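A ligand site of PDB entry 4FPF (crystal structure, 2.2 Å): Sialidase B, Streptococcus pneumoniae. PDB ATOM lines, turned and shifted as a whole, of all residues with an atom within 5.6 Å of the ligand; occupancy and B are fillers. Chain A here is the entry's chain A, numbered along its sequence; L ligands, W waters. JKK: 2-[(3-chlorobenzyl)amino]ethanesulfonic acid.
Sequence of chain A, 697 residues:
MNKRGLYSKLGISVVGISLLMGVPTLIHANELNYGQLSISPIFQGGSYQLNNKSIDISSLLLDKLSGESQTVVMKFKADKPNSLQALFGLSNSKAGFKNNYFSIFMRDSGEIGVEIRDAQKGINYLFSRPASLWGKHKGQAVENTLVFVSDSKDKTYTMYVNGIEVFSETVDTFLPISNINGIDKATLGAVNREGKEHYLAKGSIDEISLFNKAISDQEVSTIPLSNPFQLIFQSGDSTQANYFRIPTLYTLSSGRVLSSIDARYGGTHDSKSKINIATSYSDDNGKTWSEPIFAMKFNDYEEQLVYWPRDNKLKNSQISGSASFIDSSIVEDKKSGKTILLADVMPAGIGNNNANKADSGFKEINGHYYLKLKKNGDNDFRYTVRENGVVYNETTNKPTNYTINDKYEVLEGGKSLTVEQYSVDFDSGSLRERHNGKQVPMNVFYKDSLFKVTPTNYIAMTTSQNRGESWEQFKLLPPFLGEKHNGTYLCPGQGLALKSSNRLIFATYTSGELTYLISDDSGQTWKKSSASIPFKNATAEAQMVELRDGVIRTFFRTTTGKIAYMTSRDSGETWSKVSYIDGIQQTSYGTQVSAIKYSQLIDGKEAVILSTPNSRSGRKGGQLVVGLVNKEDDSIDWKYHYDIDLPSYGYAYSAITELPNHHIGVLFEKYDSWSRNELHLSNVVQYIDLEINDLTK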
ATOM      1  N   ARG A 245      29.485 -28.611  20.697  1.00  0.00           N
ATOM      2  CA  ARG A 245      28.505 -28.356  19.650  1.00  0.00           C
ATOM      3  C   ARG A 245      28.262 -26.868  19.544  1.00  0.00           C
ATOM      4  O   ARG A 245      28.630 -26.096  20.445  1.00  0.00           O
ATOM      5  CB  ARG A 245      27.181 -29.080  19.935  1.00  0.00           C
ATOM      6  CG  ARG A 245      27.130 -30.544  19.471  1.00  0.00           C
ATOM      7  CD  ARG A 245      25.682 -30.972  19.100  1.00  0.00           C
ATOM      8  NE  ARG A 245      25.131 -30.108  18.053  1.00  0.00           N
ATOM      9  CZ  ARG A 245      23.857 -30.134  17.641  1.00  0.00           C
ATOM     10  NH1 ARG A 245      22.978 -31.001  18.168  1.00  0.00           N
ATOM     11  NH2 ARG A 245      23.479 -29.310  16.677  1.00  0.00           N
ATOM     12  N   ILE A 246      27.614 -26.459  18.458  1.00  0.00           N
ATOM     13  CA  ILE A 246      27.140 -25.095  18.291  1.00  0.00           C
ATOM     14  C   ILE A 246      28.305 -24.078  18.214  1.00  0.00           C
ATOM     15  O   ILE A 246      28.442 -23.216  19.083  1.00  0.00           O
ATOM     16  CB  ILE A 246      26.162 -24.678  19.434  1.00  0.00           C
ATOM     17  CG1 ILE A 246      25.260 -25.851  19.883  1.00  0.00           C
ATOM     18  CG2 ILE A 246      25.349 -23.480  19.004  1.00  0.00           C
ATOM     19  CD1 ILE A 246      24.391 -26.467  18.794  1.00  0.00           C
ATOM     20  N   ASP A 270      21.544 -31.988  23.847  1.00  0.00           N
ATOM     21  CA  ASP A 270      21.034 -30.663  24.233  1.00  0.00           C
ATOM     22  C   ASP A 270      20.631 -30.779  25.703  1.00  0.00           C
ATOM     23  O   ASP A 270      20.333 -31.877  26.169  1.00  0.00           O
ATOM     24  CB  ASP A 270      19.750 -30.319  23.458  1.00  0.00           C
ATOM     25  CG  ASP A 270      20.001 -29.811  22.040  1.00  0.00           C
ATOM     26  OD1 ASP A 270      18.996 -29.466  21.369  1.00  0.00           O
ATOM     27  OD2 ASP A 270      21.170 -29.740  21.589  1.00  0.00           O
ATOM     28  N   SER A 271      20.624 -29.675  26.442  1.00  0.00           N
ATOM     29  CA  SER A 271      20.056 -29.711  27.788  1.00  0.00           C
ATOM     30  C   SER A 271      18.723 -30.495  27.813  1.00  0.00           C
ATOM     31  O   SER A 271      17.939 -30.387  26.878  1.00  0.00           O
ATOM     32  CB  SER A 271      19.861 -28.287  28.306  1.00  0.00           C
ATOM     33  OG  SER A 271      21.029 -27.525  28.092  1.00  0.00           O
ATOM     34  N   LYS A 272      18.451 -31.287  28.860  1.00  0.00           N
ATOM     35  CA  LYS A 272      19.217 -31.338  30.103  1.00  0.00           C
ATOM     36  C   LYS A 272      20.563 -32.084  30.049  1.00  0.00           C
ATOM     37  O   LYS A 272      20.698 -33.185  29.487  1.00  0.00           O
ATOM     38  CB  LYS A 272      18.346 -31.896  31.239  1.00  0.00           C
ATOM     39  CG  LYS A 272      17.870 -33.333  31.056  1.00  0.00           C
ATOM     40  CD  LYS A 272      16.782 -33.656  32.084  1.00  0.00           C
ATOM     41  CE  LYS A 272      16.518 -35.169  32.222  1.00  0.00           C
ATOM     42  NZ  LYS A 272      16.080 -35.858  30.956  1.00  0.00           N
ATOM     43  N   ILE A 326      23.334 -22.958  26.775  1.00  0.00           N
ATOM     44  CA  ILE A 326      23.221 -23.593  25.454  1.00  0.00           C
ATOM     45  C   ILE A 326      22.961 -22.527  24.389  1.00  0.00           C
ATOM     46  O   ILE A 326      22.256 -21.566  24.669  1.00  0.00           O
ATOM     47  CB  ILE A 326      22.104 -24.689  25.429  1.00  0.00           C
ATOM     48  CG1 ILE A 326      22.040 -25.394  24.077  1.00  0.00           C
ATOM     49  CG2 ILE A 326      20.726 -24.119  25.802  1.00  0.00           C
ATOM     50  CD1 ILE A 326      21.197 -26.681  24.135  1.00  0.00           C
ATOM     51  N   ASP A 327      23.550 -22.685  23.207  1.00  0.00           N
ATOM     52  CA  ASP A 327      23.349 -21.748  22.096  1.00  0.00           C
ATOM     53  C   ASP A 327      23.898 -20.329  22.359  1.00  0.00           C
ATOM     54  O   ASP A 327      23.188 -19.457  22.855  1.00  0.00           O
ATOM     55  CB  ASP A 327      21.867 -21.655  21.704  1.00  0.00           C
ATOM     56  CG  ASP A 327      21.334 -22.921  21.062  1.00  0.00           C
ATOM     57  OD1 ASP A 327      22.144 -23.836  20.772  1.00  0.00           O
ATOM     58  OD2 ASP A 327      20.112 -22.994  20.831  1.00  0.00           O
ATOM     59  N   ASP A 344      21.452 -19.080  25.847  1.00  0.00           N
ATOM     60  CA  ASP A 344      20.303 -19.529  26.642  1.00  0.00           C
ATOM     61  C   ASP A 344      20.795 -20.041  27.997  1.00  0.00           C
ATOM     62  O   ASP A 344      21.896 -20.574  28.104  1.00  0.00           O
ATOM     63  CB  ASP A 344      19.522 -20.654  25.953  1.00  0.00           C
ATOM     64  CG  ASP A 344      18.972 -20.258  24.587  1.00  0.00           C
ATOM     65  OD1 ASP A 344      18.708 -19.058  24.342  1.00  0.00           O
ATOM     66  OD2 ASP A 344      18.792 -21.165  23.746  1.00  0.00           O
ATOM     67  N   MET A 346      19.560 -22.475  31.426  1.00  0.00           N
ATOM     68  CA  MET A 346      18.605 -23.466  31.900  1.00  0.00           C
ATOM     69  C   MET A 346      18.891 -23.836  33.344  1.00  0.00           C
ATOM     70  O   MET A 346      20.013 -24.226  33.668  1.00  0.00           O
ATOM     71  CB  MET A 346      18.730 -24.733  31.073  1.00  0.00           C
ATOM     72  CG  MET A 346      18.745 -24.469  29.609  1.00  0.00           C
ATOM     73  SD  MET A 346      17.078 -24.569  28.974  1.00  0.00           S
ATOM     74  CE  MET A 346      17.376 -25.839  27.775  1.00  0.00           C
ATOM     75  N   GLY A 351      15.340 -28.664  30.182  1.00  0.00           N
ATOM     76  CA  GLY A 351      15.603 -28.541  28.755  1.00  0.00           C
ATOM     77  C   GLY A 351      14.475 -27.744  28.116  1.00  0.00           C
ATOM     78  O   GLY A 351      13.779 -27.014  28.813  1.00  0.00           O
ATOM     79  N   ASN A 352      14.302 -27.875  26.812  1.00  0.00           N
ATOM     80  CA  ASN A 352      13.204 -27.174  26.152  1.00  0.00           C
ATOM     81  C   ASN A 352      11.907 -27.998  26.152  1.00  0.00           C
ATOM     82  O   ASN A 352      10.818 -27.480  25.876  1.00  0.00           O
ATOM     83  CB  ASN A 352      13.590 -26.684  24.730  1.00  0.00           C
ATOM     84  CG  ASN A 352      13.633 -27.805  23.684  1.00  0.00           C
ATOM     85  OD1 ASN A 352      13.630 -28.991  24.018  1.00  0.00           O
ATOM     86  ND2 ASN A 352      13.691 -27.422  22.411  1.00  0.00           N
ATOM     87  N   ASN A 353      12.036 -29.280  26.507  1.00  0.00           N
ATOM     88  CA  ASN A 353      10.904 -30.199  26.612  1.00  0.00           C
ATOM     89  C   ASN A 353      10.125 -30.077  27.916  1.00  0.00           C
ATOM     90  O   ASN A 353       8.900 -30.230  27.951  1.00  0.00           O
ATOM     91  CB  ASN A 353      11.369 -31.647  26.440  1.00  0.00           C
ATOM     92  CG  ASN A 353      11.689 -31.991  24.994  1.00  0.00           C
ATOM     93  OD1 ASN A 353      11.169 -31.359  24.063  1.00  0.00           O
ATOM     94  ND2 ASN A 353      12.539 -32.991  24.793  1.00  0.00           N
ATOM     95  N   TYR A 489      14.177 -18.126  22.156  1.00  0.00           N
ATOM     96  CA  TYR A 489      15.407 -18.900  22.039  1.00  0.00           C
ATOM     97  C   TYR A 489      16.450 -18.167  21.196  1.00  0.00           C
ATOM     98  O   TYR A 489      16.191 -17.808  20.048  1.00  0.00           O
ATOM     99  CB  TYR A 489      15.109 -20.277  21.440  1.00  0.00           C
ATOM    100  CG  TYR A 489      14.366 -21.188  22.398  1.00  0.00           C
ATOM    101  CD1 TYR A 489      15.054 -21.926  23.344  1.00  0.00           C
ATOM    102  CD2 TYR A 489      12.975 -21.294  22.360  1.00  0.00           C
ATOM    103  CE1 TYR A 489      14.392 -22.740  24.236  1.00  0.00           C
ATOM    104  CE2 TYR A 489      12.299 -22.107  23.250  1.00  0.00           C
ATOM    105  CZ  TYR A 489      13.017 -22.834  24.190  1.00  0.00           C
ATOM    106  OH  TYR A 489      12.374 -23.657  25.094  1.00  0.00           O
ATOM    107  N   TYR A 509      14.177 -16.762  18.405  1.00  0.00           N
ATOM    108  CA  TYR A 509      12.952 -17.345  17.857  1.00  0.00           C
ATOM    109  C   TYR A 509      12.012 -17.879  18.933  1.00  0.00           C
ATOM    110  O   TYR A 509      12.419 -18.238  20.038  1.00  0.00           O
ATOM    111  CB  TYR A 509      13.257 -18.452  16.841  1.00  0.00           C
ATOM    112  CG  TYR A 509      13.911 -19.707  17.417  1.00  0.00           C
ATOM    113  CD1 TYR A 509      13.150 -20.796  17.818  1.00  0.00           C
ATOM    114  CD2 TYR A 509      15.298 -19.789  17.535  1.00  0.00           C
ATOM    115  CE1 TYR A 509      13.755 -21.957  18.343  1.00  0.00           C
ATOM    116  CE2 TYR A 509      15.900 -20.929  18.038  1.00  0.00           C
ATOM    117  CZ  TYR A 509      15.133 -22.010  18.438  1.00  0.00           C
ATOM    118  OH  TYR A 509      15.756 -23.130  18.953  1.00  0.00           O
ATOM    119  N   THR A 539      12.184 -24.571  14.694  1.00  0.00           N
ATOM    120  CA  THR A 539      13.467 -24.198  15.269  1.00  0.00           C
ATOM    121  C   THR A 539      14.057 -23.197  14.279  1.00  0.00           C
ATOM    122  O   THR A 539      14.891 -23.553  13.468  1.00  0.00           O
ATOM    123  CB  THR A 539      14.375 -25.436  15.421  1.00  0.00           C
ATOM    124  OG1 THR A 539      13.651 -26.482  16.076  1.00  0.00           O
ATOM    125  CG2 THR A 539      15.627 -25.094  16.226  1.00  0.00           C
ATOM    126  N   GLU A 541      16.262 -20.988  13.637  1.00  0.00           N
ATOM    127  CA  GLU A 541      17.584 -20.413  13.854  1.00  0.00           C
ATOM    128  C   GLU A 541      17.909 -19.488  12.695  1.00  0.00           C
ATOM    129  O   GLU A 541      17.917 -19.907  11.528  1.00  0.00           O
ATOM    130  CB  GLU A 541      18.630 -21.521  14.015  1.00  0.00           C
ATOM    131  CG  GLU A 541      18.423 -22.331  15.283  1.00  0.00           C
ATOM    132  CD  GLU A 541      19.009 -23.728  15.213  1.00  0.00           C
ATOM    133  OE1 GLU A 541      19.227 -24.327  16.299  1.00  0.00           O
ATOM    134  OE2 GLU A 541      19.263 -24.209  14.099  1.00  0.00           O
ATOM    135  N   ARG A 557      16.361 -21.225   9.336  1.00  0.00           N
ATOM    136  CA  ARG A 557      15.992 -22.630   9.295  1.00  0.00           C
ATOM    137  C   ARG A 557      14.480 -22.762   9.416  1.00  0.00           C
ATOM    138  O   ARG A 557      13.847 -22.035  10.171  1.00  0.00           O
ATOM    139  CB  ARG A 557      16.647 -23.320  10.487  1.00  0.00           C
ATOM    140  CG  ARG A 557      16.343 -24.786  10.638  1.00  0.00           C
ATOM    141  CD  ARG A 557      16.929 -25.295  11.934  1.00  0.00           C
ATOM    142  NE  ARG A 557      16.450 -26.631  12.259  1.00  0.00           N
ATOM    143  CZ  ARG A 557      16.939 -27.357  13.262  1.00  0.00           C
ATOM    144  NH1 ARG A 557      17.916 -26.872  14.018  1.00  0.00           N
ATOM    145  NH2 ARG A 557      16.458 -28.577  13.501  1.00  0.00           N
ATOM    146  N   GLY A 590      15.517 -29.554   9.378  1.00  0.00           N
ATOM    147  CA  GLY A 590      16.365 -28.420   9.056  1.00  0.00           C
ATOM    148  C   GLY A 590      17.634 -28.333   9.897  1.00  0.00           C
ATOM    149  O   GLY A 590      17.805 -29.068  10.862  1.00  0.00           O
ATOM    150  N   ARG A 619      22.199 -34.447   7.648  1.00  0.00           N
ATOM    151  CA  ARG A 619      23.121 -33.335   7.820  1.00  0.00           C
ATOM    152  C   ARG A 619      24.481 -33.712   7.254  1.00  0.00           C
ATOM    153  O   ARG A 619      25.381 -34.153   7.958  1.00  0.00           O
ATOM    154  CB  ARG A 619      23.208 -32.947   9.302  1.00  0.00           C
ATOM    155  CG  ARG A 619      21.857 -32.422   9.831  1.00  0.00           C
ATOM    156  CD  ARG A 619      21.959 -31.924  11.259  1.00  0.00           C
ATOM    157  NE  ARG A 619      20.817 -31.091  11.636  1.00  0.00           N
ATOM    158  CZ  ARG A 619      20.540 -30.765  12.897  1.00  0.00           C
ATOM    159  NH1 ARG A 619      21.326 -31.205  13.890  1.00  0.00           N
ATOM    160  NH2 ARG A 619      19.490 -30.000  13.177  1.00  0.00           N
ATOM    161  N   TYR A 653      25.762 -27.923  12.155  1.00  0.00           N
ATOM    162  CA  TYR A 653      25.821 -26.506  12.512  1.00  0.00           C
ATOM    163  C   TYR A 653      27.159 -25.925  12.075  1.00  0.00           C
ATOM    164  O   TYR A 653      28.169 -26.632  12.049  1.00  0.00           O
ATOM    165  CB  TYR A 653      25.642 -26.286  14.012  1.00  0.00           C
ATOM    166  CG  TYR A 653      24.215 -26.318  14.491  1.00  0.00           C
ATOM    167  CD1 TYR A 653      23.328 -27.310  14.064  1.00  0.00           C
ATOM    168  CD2 TYR A 653      23.745 -25.379  15.405  1.00  0.00           C
ATOM    169  CE1 TYR A 653      22.018 -27.353  14.517  1.00  0.00           C
ATOM    170  CE2 TYR A 653      22.442 -25.416  15.868  1.00  0.00           C
ATOM    171  CZ  TYR A 653      21.572 -26.410  15.413  1.00  0.00           C
ATOM    172  OH  TYR A 653      20.275 -26.454  15.878  1.00  0.00           O
ATOM    173  N   SER A 673      24.728 -34.215  13.430  1.00  0.00           N
ATOM    174  CA  SER A 673      24.328 -33.973  14.822  1.00  0.00           C
ATOM    175  C   SER A 673      22.829 -34.179  15.069  1.00  0.00           C
ATOM    176  O   SER A 673      22.313 -33.882  16.162  1.00  0.00           O
ATOM    177  CB  SER A 673      24.766 -32.579  15.275  1.00  0.00           C
ATOM    178  OG  SER A 673      24.199 -31.561  14.469  1.00  0.00           O
ATOM    179  N   TRP A 674      22.114 -34.656  14.051  1.00  0.00           N
ATOM    180  CA  TRP A 674      20.727 -35.081  14.233  1.00  0.00           C
ATOM    181  C   TRP A 674      20.689 -36.588  14.458  1.00  0.00           C
ATOM    182  O   TRP A 674      19.952 -37.078  15.304  1.00  0.00           O
ATOM    183  CB  TRP A 674      19.870 -34.723  13.004  1.00  0.00           C
ATOM    184  CG  TRP A 674      18.396 -34.969  13.205  1.00  0.00           C
ATOM    185  CD1 TRP A 674      17.691 -36.087  12.838  1.00  0.00           C
ATOM    186  CD2 TRP A 674      17.442 -34.084  13.833  1.00  0.00           C
ATOM    187  NE1 TRP A 674      16.359 -35.941  13.187  1.00  0.00           N
ATOM    188  CE2 TRP A 674      16.186 -34.722  13.789  1.00  0.00           C
ATOM    189  CE3 TRP A 674      17.540 -32.811  14.414  1.00  0.00           C
ATOM    190  CZ2 TRP A 674      15.035 -34.137  14.308  1.00  0.00           C
ATOM    191  CZ3 TRP A 674      16.399 -32.221  14.914  1.00  0.00           C
ATOM    192  CH2 TRP A 674      15.155 -32.888  14.872  1.00  0.00           C
HETATM  193  CAE JKK L   1      17.719 -24.389  23.555  1.00  0.00           C
HETATM  194  CAF JKK L   1      17.552 -25.402  24.475  1.00  0.00           C
HETATM  195  CAG JKK L   1      17.664 -24.698  22.163  1.00  0.00           C
HETATM  196  CAH JKK L   1      17.279 -26.957  22.729  1.00  0.00           C
HETATM  197  CAI JKK L   1      18.363 -27.770  18.635  1.00  0.00           C
HETATM  198  CAJ JKK L   1      19.593 -28.524  18.123  1.00  0.00           C
HETATM  199  CAK JKK L   1      17.390 -26.331  20.260  1.00  0.00           C
HETATM  200  CAM JKK L   1      17.337 -26.664  24.092  1.00  0.00           C
HETATM  201  CAN JKK L   1      17.442 -25.937  21.798  1.00  0.00           C
HETATM  202  NAL JKK L   1      18.583 -27.001  19.810  1.00  0.00           N
HETATM  203  OAA JKK L   1      18.433 -30.806  17.530  1.00  0.00           O
HETATM  204  OAB JKK L   1      18.626 -29.236  15.727  1.00  0.00           O
HETATM  205  OAC JKK L   1      20.578 -30.397  16.512  1.00  0.00           O
HETATM  206  SAO JKK L   1      19.292 -29.799  16.914  1.00  0.00           S
HETATM  207 CL   JKK L   1      17.123 -27.934  25.212  1.00  0.00          CL
HETATM  208  O   HOH W   1      18.396 -23.528  18.549  1.00  0.00           O
HETATM  209  O   HOH W   2      20.863 -26.017  19.776  1.00  0.00           O
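NH1 of Arg 619 is in hydrogen-bond range of OG of Ser 673 (3.0 Å).
NH2 of Arg 245 sits at hydrogen-bond distance from OG of Ser 673, 3.2 Å away.
NH1 of Arg 557 is in salt-bridge range of OE2 of Glu 541 (3.0 Å).
The guanidinium group of Arg 557 is in hydrogen-bond range of the backbone carbonyl oxygen of Gly 590 (3.0 Å).
OD1 of Asn 352 lies close to OD1 of Asn 353, at 3.4 Å.
O of Asp 327 is in hydrogen-bond range of N of Asp 344, 3.5 Å away.
O of Ile 326 lies within hydrogen-bond range of N of Asp 344 (2.9 Å).
N of Tyr 489 sits at hydrogen-bond distance from O of Tyr 509, 2.8 Å away.
O of Ser 271 touches CL of the ligand, at 3.1 Å.
CG2 of Ile 326 touches CAF of the ligand, 3.7 Å away.
OD2 of Asp 327 touches CAG of the ligand, 3.3 Å away.
Asp 344 touches the ligand.
Met 346 touches the ligand (CE to CL, 3.3 Å).
Gly 351 touches the ligand (CA to CL, 3.9 Å).
Asn 352 touches the ligand.
Tyr 489 touches the ligand.
Tyr 509 touches the ligand.
O of Ser 673 touches OAC of the ligand (3.9 Å).
Trp 674 touches the ligand.
Hydrophobic or aromatic side chains within 4 Å of the ligand: Ile 326, Met 346, Tyr 489, Tyr 653 and Trp 674.
An oxygen (OAB) of the ligand is in salt-bridge range of the guanidinium group of Arg 619.
A nitrogen (NAL) of the ligand is in salt-bridge range of the side-chain carboxylate of Asp 270, 2.9 Å away.
The guanidinium group of Arg 245 is in salt-bridge range of an oxygen (OAC) of the ligand, at 3.0 Å.
The guanidinium group (NH1) of Arg 557 is in salt-bridge range of an oxygen (OAB) of the ligand (3.0 Å).
The side-chain hydroxyl of Tyr 653 lies close to an oxygen (OAB) of the ligand.
Water W2 lies within hydrogen-bond range of a nitrogen (NAL) of the ligand and the side-chain carboxylate of Asp 327.
Water W1 lies within hydrogen-bond range of OE1 of Glu 541 (2.5 Å), OH of Tyr 509 (2.7 Å) and OD2 of Asp 327 (2.9 Å).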
